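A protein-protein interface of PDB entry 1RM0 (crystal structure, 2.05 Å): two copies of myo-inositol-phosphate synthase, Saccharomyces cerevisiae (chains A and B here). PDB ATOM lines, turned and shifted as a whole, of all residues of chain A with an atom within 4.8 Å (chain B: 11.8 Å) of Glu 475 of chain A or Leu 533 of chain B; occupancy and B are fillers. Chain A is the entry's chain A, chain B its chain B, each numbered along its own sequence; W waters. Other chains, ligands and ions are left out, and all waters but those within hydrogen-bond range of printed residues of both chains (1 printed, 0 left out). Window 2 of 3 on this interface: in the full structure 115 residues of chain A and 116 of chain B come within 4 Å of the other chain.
Leu 533 of chain B touches just these residues of chain A: Tyr 461, Lys 463, Glu 475, Asn 476, Tyr 478 and Arg 494.
No residue of chain B comes within 4 Å of Ser 460 of chain A.
Of chain B, only Leu 532 and Leu 533 come within 4 Å of Tyr 461 of chain A.
No residue of chain B comes within 4 Å of Lys 473 of chain A.
No residue of chain B comes within 4 Å of Phe 474 of chain A.
Tyr 478 of chain A touches just these residues of chain B: Glu 530 (3.8 Å), Arg 531 (2.9 Å) and Leu 533 (3.6 Å).
Of the printed residues of chain A, Leu 532 of chain B touches Tyr 461, Phe 477 and Arg 494.
Of the printed residues of chain B, Arg 494 of chain A touches Glu 529 (3.9 Å), Glu 530 (2.9 Å), Leu 532 (2.8 Å) and Leu 533 (3.7 Å).
Arg 527 of chain B touches none of the printed residues of chain A.
The nearest printed residue of chain A that does not touch Glu 530 of chain B is Phe 477 of chain A (6.8 Å).
OH of Tyr 461 of chain A touches CA of Leu 532 of chain B (3.4 Å).
CD1 of Leu 533 of chain B touches OE1 of Glu 475 of chain A, 3.8 Å away.
Leu 533 of chain B touches Asn 476 of chain A.
CD1 of Phe 477 of chain A touches O of Arg 531 of chain B, at 3.8 Å.
CD2 of Leu 532 of chain B touches CD1 of Phe 477 of chain A (3.9 Å).
Glu 530 of chain B touches Tyr 478 of chain A (O to CB, 3.8 Å).
Leu 533 of chain B touches Tyr 478 of chain A.
Glu 529 of chain B touches Arg 494 of chain A.
Water W1 lies within hydrogen-bond range of O of Arg 531 of chain B and O of Tyr 478 of chain A.
The backbone NH (N) of Leu 533 of chain B is in hydrogen-bond range of the side-chain hydroxyl (OH) of Tyr 461 of chain A (2.8 Å).
The side-chain amino group (NZ) of Lys 463 of chain A lies within salt-bridge range of the chain-end carboxylate (OXT) of Leu 533 of chain B, 3.96 Å away.
N of Tyr 478 of chain A is in hydrogen-bond range of O of Arg 531 of chain B.
The guanidinium group (NH1) of Arg 494 of chain A is in hydrogen-bond range of the backbone carbonyl oxygen (O) of Glu 530 of chain B.
NH1 of Arg 494 of chain A lies within hydrogen-bond range of O of Leu 532 of chain B, at 2.8 Å.
The guanidinium group of Arg 494 of chain A lies within salt-bridge range of the chain-end carboxylate of Leu 533 of chain B (3.7 Å).
Of the 9 printed residues of chain B, 5 touch a printed residue of chain A.
Printed residues of chain B that touch a printed residue of chain A: Glu 529, Glu 530, Arg 531, Leu 532 and Leu 533.
Hydrophobic or aromatic side chains of chain B within 4 Å of the printed part of chain A: Leu 532 and Leu 533.
Hydrophobic or aromatic side chains of chain A within 4 Å of the printed part of chain B: Tyr 461, Phe 477 and Tyr 478.
Among the printed residues, 14 pairs touch across the chains.
No position is printed for both chains.
O of Val 459 of chain A sits close to OD1 of Asn 476 of chain A (3.2 Å).
The backbone NH (N) of Glu 475 of chain A sits at hydrogen-bond distance from the backbone carbonyl oxygen (O) of Tyr 461 of chain A, 2.6 Å away.
The side-chain hydroxyl of Tyr 461 of chain A is in hydrogen-bond range of the backbone carbonyl oxygen of Asn 476 of chain A, at 2.9 Å.
The side-chain amino group of Lys 473 of chain A is in salt-bridge range of the side-chain carboxylate of Glu 475 of chain A, at 3.0 Å.
NE of Arg 531 of chain B sits at hydrogen-bond distance from O of Leu 526 of chain B (2.7 Å).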
ATOM      1  N   VAL A 459      36.845  16.136  -6.158  1.00  0.00           N
ATOM      2  CA  VAL A 459      35.842  15.578  -7.052  1.00  0.00           C
ATOM      3  C   VAL A 459      35.352  16.608  -8.064  1.00  0.00           C
ATOM      4  O   VAL A 459      35.100  17.765  -7.709  1.00  0.00           O
ATOM      5  CB  VAL A 459      34.602  15.087  -6.261  1.00  0.00           C
ATOM      6  CG1 VAL A 459      33.495  14.662  -7.231  1.00  0.00           C
ATOM      7  CG2 VAL A 459      34.991  13.942  -5.329  1.00  0.00           C
ATOM      8  N   SER A 460      35.224  16.182  -9.322  1.00  0.00           N
ATOM      9  CA  SER A 460      34.703  17.037 -10.392  1.00  0.00           C
ATOM     10  C   SER A 460      33.900  16.119 -11.301  1.00  0.00           C
ATOM     11  O   SER A 460      33.985  14.894 -11.189  1.00  0.00           O
ATOM     12  CB  SER A 460      35.822  17.735 -11.183  1.00  0.00           C
ATOM     13  OG  SER A 460      36.619  16.820 -11.908  1.00  0.00           O
ATOM     14  N   TYR A 461      33.125  16.700 -12.204  1.00  0.00           N
ATOM     15  CA  TYR A 461      32.287  15.899 -13.087  1.00  0.00           C
ATOM     16  C   TYR A 461      31.874  16.693 -14.313  1.00  0.00           C
ATOM     17  O   TYR A 461      32.153  17.883 -14.420  1.00  0.00           O
ATOM     18  CB  TYR A 461      31.033  15.499 -12.321  1.00  0.00           C
ATOM     19  CG  TYR A 461      30.313  16.714 -11.784  1.00  0.00           C
ATOM     20  CD1 TYR A 461      29.348  17.373 -12.542  1.00  0.00           C
ATOM     21  CD2 TYR A 461      30.680  17.272 -10.561  1.00  0.00           C
ATOM     22  CE1 TYR A 461      28.775  18.564 -12.098  1.00  0.00           C
ATOM     23  CE2 TYR A 461      30.117  18.459 -10.113  1.00  0.00           C
ATOM     24  CZ  TYR A 461      29.169  19.101 -10.886  1.00  0.00           C
ATOM     25  OH  TYR A 461      28.636  20.287 -10.446  1.00  0.00           O
ATOM     26  N   LYS A 463      28.508  16.593 -17.448  1.00  0.00           N
ATOM     27  CA  LYS A 463      27.357  15.918 -18.037  1.00  0.00           C
ATOM     28  C   LYS A 463      27.833  15.203 -19.295  1.00  0.00           C
ATOM     29  O   LYS A 463      28.731  15.678 -19.991  1.00  0.00           O
ATOM     30  CB  LYS A 463      26.260  16.908 -18.438  1.00  0.00           C
ATOM     31  CG  LYS A 463      25.615  17.698 -17.318  1.00  0.00           C
ATOM     32  CD  LYS A 463      24.236  18.160 -17.778  1.00  0.00           C
ATOM     33  CE  LYS A 463      23.588  19.144 -16.825  1.00  0.00           C
ATOM     34  NZ  LYS A 463      24.208  20.498 -16.915  1.00  0.00           N
ATOM     35  N   LYS A 473      32.921  20.202 -20.085  1.00  0.00           N
ATOM     36  CA  LYS A 473      34.170  20.188 -19.325  1.00  0.00           C
ATOM     37  C   LYS A 473      33.835  19.983 -17.851  1.00  0.00           C
ATOM     38  O   LYS A 473      32.745  20.340 -17.391  1.00  0.00           O
ATOM     39  CB  LYS A 473      34.930  21.506 -19.501  1.00  0.00           C
ATOM     40  CG  LYS A 473      34.393  22.659 -18.665  1.00  0.00           C
ATOM     41  CD  LYS A 473      35.226  23.918 -18.867  1.00  0.00           C
ATOM     42  CE  LYS A 473      34.875  24.990 -17.844  1.00  0.00           C
ATOM     43  NZ  LYS A 473      35.219  24.559 -16.460  1.00  0.00           N
ATOM     44  N   PHE A 474      34.777  19.418 -17.107  1.00  0.00           N
ATOM     45  CA  PHE A 474      34.545  19.155 -15.699  1.00  0.00           C
ATOM     46  C   PHE A 474      34.238  20.373 -14.861  1.00  0.00           C
ATOM     47  O   PHE A 474      34.799  21.444 -15.060  1.00  0.00           O
ATOM     48  CB  PHE A 474      35.726  18.409 -15.099  1.00  0.00           C
ATOM     49  CG  PHE A 474      35.886  17.021 -15.634  1.00  0.00           C
ATOM     50  CD1 PHE A 474      36.649  16.783 -16.764  1.00  0.00           C
ATOM     51  CD2 PHE A 474      35.258  15.950 -15.015  1.00  0.00           C
ATOM     52  CE1 PHE A 474      36.787  15.493 -17.269  1.00  0.00           C
ATOM     53  CE2 PHE A 474      35.392  14.658 -15.514  1.00  0.00           C
ATOM     54  CZ  PHE A 474      36.158  14.429 -16.641  1.00  0.00           C
ATOM     55  N   GLU A 475      33.318  20.189 -13.927  1.00  0.00           N
ATOM     56  CA  GLU A 475      32.903  21.235 -13.008  1.00  0.00           C
ATOM     57  C   GLU A 475      33.103  20.694 -11.601  1.00  0.00           C
ATOM     58  O   GLU A 475      33.401  19.513 -11.415  1.00  0.00           O
ATOM     59  CB  GLU A 475      31.424  21.566 -13.210  1.00  0.00           C
ATOM     60  CG  GLU A 475      31.098  22.185 -14.545  1.00  0.00           C
ATOM     61  CD  GLU A 475      31.823  23.489 -14.745  1.00  0.00           C
ATOM     62  OE1 GLU A 475      31.747  24.348 -13.842  1.00  0.00           O
ATOM     63  OE2 GLU A 475      32.467  23.657 -15.800  1.00  0.00           O
ATOM     64  N   ASN A 476      32.952  21.562 -10.611  1.00  0.00           N
ATOM     65  CA  ASN A 476      33.081  21.133  -9.230  1.00  0.00           C
ATOM     66  C   ASN A 476      31.700  21.168  -8.621  1.00  0.00           C
ATOM     67  O   ASN A 476      30.772  21.722  -9.207  1.00  0.00           O
ATOM     68  CB  ASN A 476      34.003  22.063  -8.453  1.00  0.00           C
ATOM     69  CG  ASN A 476      35.455  21.824  -8.769  1.00  0.00           C
ATOM     70  OD1 ASN A 476      35.961  20.710  -8.620  1.00  0.00           O
ATOM     71  ND2 ASN A 476      36.139  22.866  -9.210  1.00  0.00           N
ATOM     72  N   PHE A 477      31.563  20.568  -7.451  1.00  0.00           N
ATOM     73  CA  PHE A 477      30.284  20.545  -6.760  1.00  0.00           C
ATOM     74  C   PHE A 477      29.695  21.940  -6.682  1.00  0.00           C
ATOM     75  O   PHE A 477      30.433  22.926  -6.641  1.00  0.00           O
ATOM     76  CB  PHE A 477      30.472  20.024  -5.338  1.00  0.00           C
ATOM     77  CG  PHE A 477      30.494  18.536  -5.240  1.00  0.00           C
ATOM     78  CD1 PHE A 477      29.331  17.802  -5.427  1.00  0.00           C
ATOM     79  CD2 PHE A 477      31.672  17.863  -4.954  1.00  0.00           C
ATOM     80  CE1 PHE A 477      29.342  16.421  -5.327  1.00  0.00           C
ATOM     81  CE2 PHE A 477      31.693  16.478  -4.852  1.00  0.00           C
ATOM     82  CZ  PHE A 477      30.526  15.759  -5.038  1.00  0.00           C
ATOM     83  N   TYR A 478      28.370  22.036  -6.682  1.00  0.00           N
ATOM     84  CA  TYR A 478      27.762  23.345  -6.528  1.00  0.00           C
ATOM     85  C   TYR A 478      28.277  23.780  -5.145  1.00  0.00           C
ATOM     86  O   TYR A 478      28.233  22.993  -4.190  1.00  0.00           O
ATOM     87  CB  TYR A 478      26.239  23.237  -6.539  1.00  0.00           C
ATOM     88  CG  TYR A 478      25.564  24.449  -5.950  1.00  0.00           C
ATOM     89  CD1 TYR A 478      25.088  24.431  -4.644  1.00  0.00           C
ATOM     90  CD2 TYR A 478      25.466  25.639  -6.671  1.00  0.00           C
ATOM     91  CE1 TYR A 478      24.530  25.569  -4.059  1.00  0.00           C
ATOM     92  CE2 TYR A 478      24.912  26.790  -6.094  1.00  0.00           C
ATOM     93  CZ  TYR A 478      24.448  26.745  -4.787  1.00  0.00           C
ATOM     94  OH  TYR A 478      23.918  27.869  -4.192  1.00  0.00           O
ATOM     95  N   PRO A 479      28.779  25.027  -5.024  1.00  0.00           N
ATOM     96  CA  PRO A 479      29.326  25.612  -3.786  1.00  0.00           C
ATOM     97  C   PRO A 479      28.792  25.103  -2.433  1.00  0.00           C
ATOM     98  O   PRO A 479      29.581  24.712  -1.565  1.00  0.00           O
ATOM     99  CB  PRO A 479      29.100  27.105  -3.994  1.00  0.00           C
ATOM    100  CG  PRO A 479      29.383  27.250  -5.451  1.00  0.00           C
ATOM    101  CD  PRO A 479      28.650  26.065  -6.065  1.00  0.00           C
ATOM    102  N   ARG A 494      20.478  24.757  -1.478  1.00  0.00           N
ATOM    103  CA  ARG A 494      20.601  25.582  -2.670  1.00  0.00           C
ATOM    104  C   ARG A 494      19.308  26.383  -2.780  1.00  0.00           C
ATOM    105  O   ARG A 494      18.222  25.867  -2.498  1.00  0.00           O
ATOM    106  CB  ARG A 494      20.777  24.684  -3.897  1.00  0.00           C
ATOM    107  CG  ARG A 494      20.863  25.401  -5.235  1.00  0.00           C
ATOM    108  CD  ARG A 494      21.346  24.431  -6.292  1.00  0.00           C
ATOM    109  NE  ARG A 494      21.684  25.086  -7.550  1.00  0.00           N
ATOM    110  CZ  ARG A 494      22.387  24.510  -8.520  1.00  0.00           C
ATOM    111  NH1 ARG A 494      22.830  23.267  -8.381  1.00  0.00           N
ATOM    112  NH2 ARG A 494      22.651  25.179  -9.631  1.00  0.00           N
ATOM    113  N   GLU B 122      10.281  22.311  -8.607  1.00  0.00           N
ATOM    114  CA  GLU B 122      11.188  23.087  -7.759  1.00  0.00           C
ATOM    115  C   GLU B 122      12.409  22.284  -7.296  1.00  0.00           C
ATOM    116  O   GLU B 122      13.406  22.856  -6.847  1.00  0.00           O
ATOM    117  CB  GLU B 122      10.432  23.619  -6.537  1.00  0.00           C
ATOM    118  CG  GLU B 122       8.941  23.841  -6.773  1.00  0.00           C
ATOM    119  CD  GLU B 122       8.648  24.822  -7.896  1.00  0.00           C
ATOM    120  OE1 GLU B 122       7.533  24.764  -8.458  1.00  0.00           O
ATOM    121  OE2 GLU B 122       9.523  25.656  -8.212  1.00  0.00           O
ATOM    122  N   LEU B 526      20.799  10.944  -4.156  1.00  0.00           N
ATOM    123  CA  LEU B 526      21.910  11.742  -4.663  1.00  0.00           C
ATOM    124  C   LEU B 526      21.544  13.188  -4.961  1.00  0.00           C
ATOM    125  O   LEU B 526      22.408  14.071  -4.935  1.00  0.00           O
ATOM    126  CB  LEU B 526      22.492  11.069  -5.901  1.00  0.00           C
ATOM    127  CG  LEU B 526      23.116   9.714  -5.559  1.00  0.00           C
ATOM    128  CD1 LEU B 526      23.480   8.973  -6.831  1.00  0.00           C
ATOM    129  CD2 LEU B 526      24.337   9.931  -4.679  1.00  0.00           C
ATOM    130  N   ARG B 527      20.266  13.427  -5.238  1.00  0.00           N
ATOM    131  CA  ARG B 527      19.774  14.769  -5.531  1.00  0.00           C
ATOM    132  C   ARG B 527      20.758  15.611  -6.323  1.00  0.00           C
ATOM    133  O   ARG B 527      21.125  16.702  -5.889  1.00  0.00           O
ATOM    134  CB  ARG B 527      19.432  15.493  -4.232  1.00  0.00           C
ATOM    135  CG  ARG B 527      18.350  14.806  -3.441  1.00  0.00           C
ATOM    136  CD  ARG B 527      18.313  15.297  -2.010  1.00  0.00           C
ATOM    137  NE  ARG B 527      17.280  14.613  -1.237  1.00  0.00           N
ATOM    138  CZ  ARG B 527      15.984  14.888  -1.325  1.00  0.00           C
ATOM    139  NH1 ARG B 527      15.559  15.842  -2.149  1.00  0.00           N
ATOM    140  NH2 ARG B 527      15.114  14.207  -0.592  1.00  0.00           N
ATOM    141  N   PHE B 528      21.180  15.113  -7.484  1.00  0.00           N
ATOM    142  CA  PHE B 528      22.118  15.851  -8.318  1.00  0.00           C
ATOM    143  C   PHE B 528      21.502  17.134  -8.886  1.00  0.00           C
ATOM    144  O   PHE B 528      22.218  18.036  -9.308  1.00  0.00           O
ATOM    145  CB  PHE B 528      22.643  14.955  -9.441  1.00  0.00           C
ATOM    146  CG  PHE B 528      23.717  13.993  -8.997  1.00  0.00           C
ATOM    147  CD1 PHE B 528      24.117  12.943  -9.822  1.00  0.00           C
ATOM    148  CD2 PHE B 528      24.342  14.140  -7.759  1.00  0.00           C
ATOM    149  CE1 PHE B 528      25.123  12.053  -9.422  1.00  0.00           C
ATOM    150  CE2 PHE B 528      25.348  13.256  -7.350  1.00  0.00           C
ATOM    151  CZ  PHE B 528      25.738  12.214  -8.182  1.00  0.00           C
ATOM    152  N   GLU B 529      20.177  17.228  -8.885  1.00  0.00           N
ATOM    153  CA  GLU B 529      19.524  18.432  -9.386  1.00  0.00           C
ATOM    154  C   GLU B 529      19.934  19.621  -8.521  1.00  0.00           C
ATOM    155  O   GLU B 529      19.837  20.775  -8.942  1.00  0.00           O
ATOM    156  CB  GLU B 529      18.003  18.285  -9.344  1.00  0.00           C
ATOM    157  CG  GLU B 529      17.439  17.261 -10.309  1.00  0.00           C
ATOM    158  CD  GLU B 529      17.626  15.834  -9.837  1.00  0.00           C
ATOM    159  OE1 GLU B 529      17.243  14.909 -10.588  1.00  0.00           O
ATOM    160  OE2 GLU B 529      18.147  15.634  -8.718  1.00  0.00           O
ATOM    161  N   GLU B 530      20.386  19.326  -7.305  1.00  0.00           N
ATOM    162  CA  GLU B 530      20.812  20.359  -6.369  1.00  0.00           C
ATOM    163  C   GLU B 530      22.324  20.357  -6.122  1.00  0.00           C
ATOM    164  O   GLU B 530      22.971  21.394  -6.216  1.00  0.00           O
ATOM    165  CB  GLU B 530      20.072  20.196  -5.032  1.00  0.00           C
ATOM    166  CG  GLU B 530      20.659  21.027  -3.888  1.00  0.00           C
ATOM    167  CD  GLU B 530      19.876  20.909  -2.584  1.00  0.00           C
ATOM    168  OE1 GLU B 530      19.494  19.777  -2.210  1.00  0.00           O
ATOM    169  OE2 GLU B 530      19.652  21.951  -1.927  1.00  0.00           O
ATOM    170  N   ARG B 531      22.882  19.189  -5.827  1.00  0.00           N
ATOM    171  CA  ARG B 531      24.307  19.076  -5.524  1.00  0.00           C
ATOM    172  C   ARG B 531      25.242  19.427  -6.676  1.00  0.00           C
ATOM    173  O   ARG B 531      26.347  19.937  -6.461  1.00  0.00           O
ATOM    174  CB  ARG B 531      24.635  17.660  -5.029  1.00  0.00           C
ATOM    175  CG  ARG B 531      23.803  17.179  -3.842  1.00  0.00           C
ATOM    176  CD  ARG B 531      24.360  15.859  -3.328  1.00  0.00           C
ATOM    177  NE  ARG B 531      23.363  15.041  -2.641  1.00  0.00           N
ATOM    178  CZ  ARG B 531      22.876  15.287  -1.430  1.00  0.00           C
ATOM    179  NH1 ARG B 531      23.290  16.339  -0.744  1.00  0.00           N
ATOM    180  NH2 ARG B 531      21.973  14.474  -0.904  1.00  0.00           N
ATOM    181  N   LEU B 532      24.813  19.140  -7.897  1.00  0.00           N
ATOM    182  CA  LEU B 532      25.643  19.433  -9.055  1.00  0.00           C
ATOM    183  C   LEU B 532      25.158  20.707  -9.743  1.00  0.00           C
ATOM    184  O   LEU B 532      23.989  21.084  -9.625  1.00  0.00           O
ATOM    185  CB  LEU B 532      25.621  18.247 -10.024  1.00  0.00           C
ATOM    186  CG  LEU B 532      25.891  16.865  -9.404  1.00  0.00           C
ATOM    187  CD1 LEU B 532      25.968  15.817 -10.508  1.00  0.00           C
ATOM    188  CD2 LEU B 532      27.194  16.874  -8.615  1.00  0.00           C
ATOM    189  N   LEU B 533      26.067  21.382 -10.438  1.00  0.00           N
ATOM    190  CA  LEU B 533      25.724  22.612 -11.143  1.00  0.00           C
ATOM    191  C   LEU B 533      24.811  22.316 -12.333  1.00  0.00           C
ATOM    192  O   LEU B 533      23.686  22.862 -12.347  1.00  0.00           O
ATOM    193  CB  LEU B 533      27.002  23.318 -11.616  1.00  0.00           C
ATOM    194  CG  LEU B 533      27.884  23.843 -10.480  1.00  0.00           C
ATOM    195  CD1 LEU B 533      29.253  24.235 -10.992  1.00  0.00           C
ATOM    196  CD2 LEU B 533      27.189  25.020  -9.828  1.00  0.00           C
ATOM    197  OXT LEU B 533      25.225  21.538 -13.227  1.00  0.00           O
HETATM  198  O   HOH W   1      26.789  20.189  -3.289  1.00  0.00           O
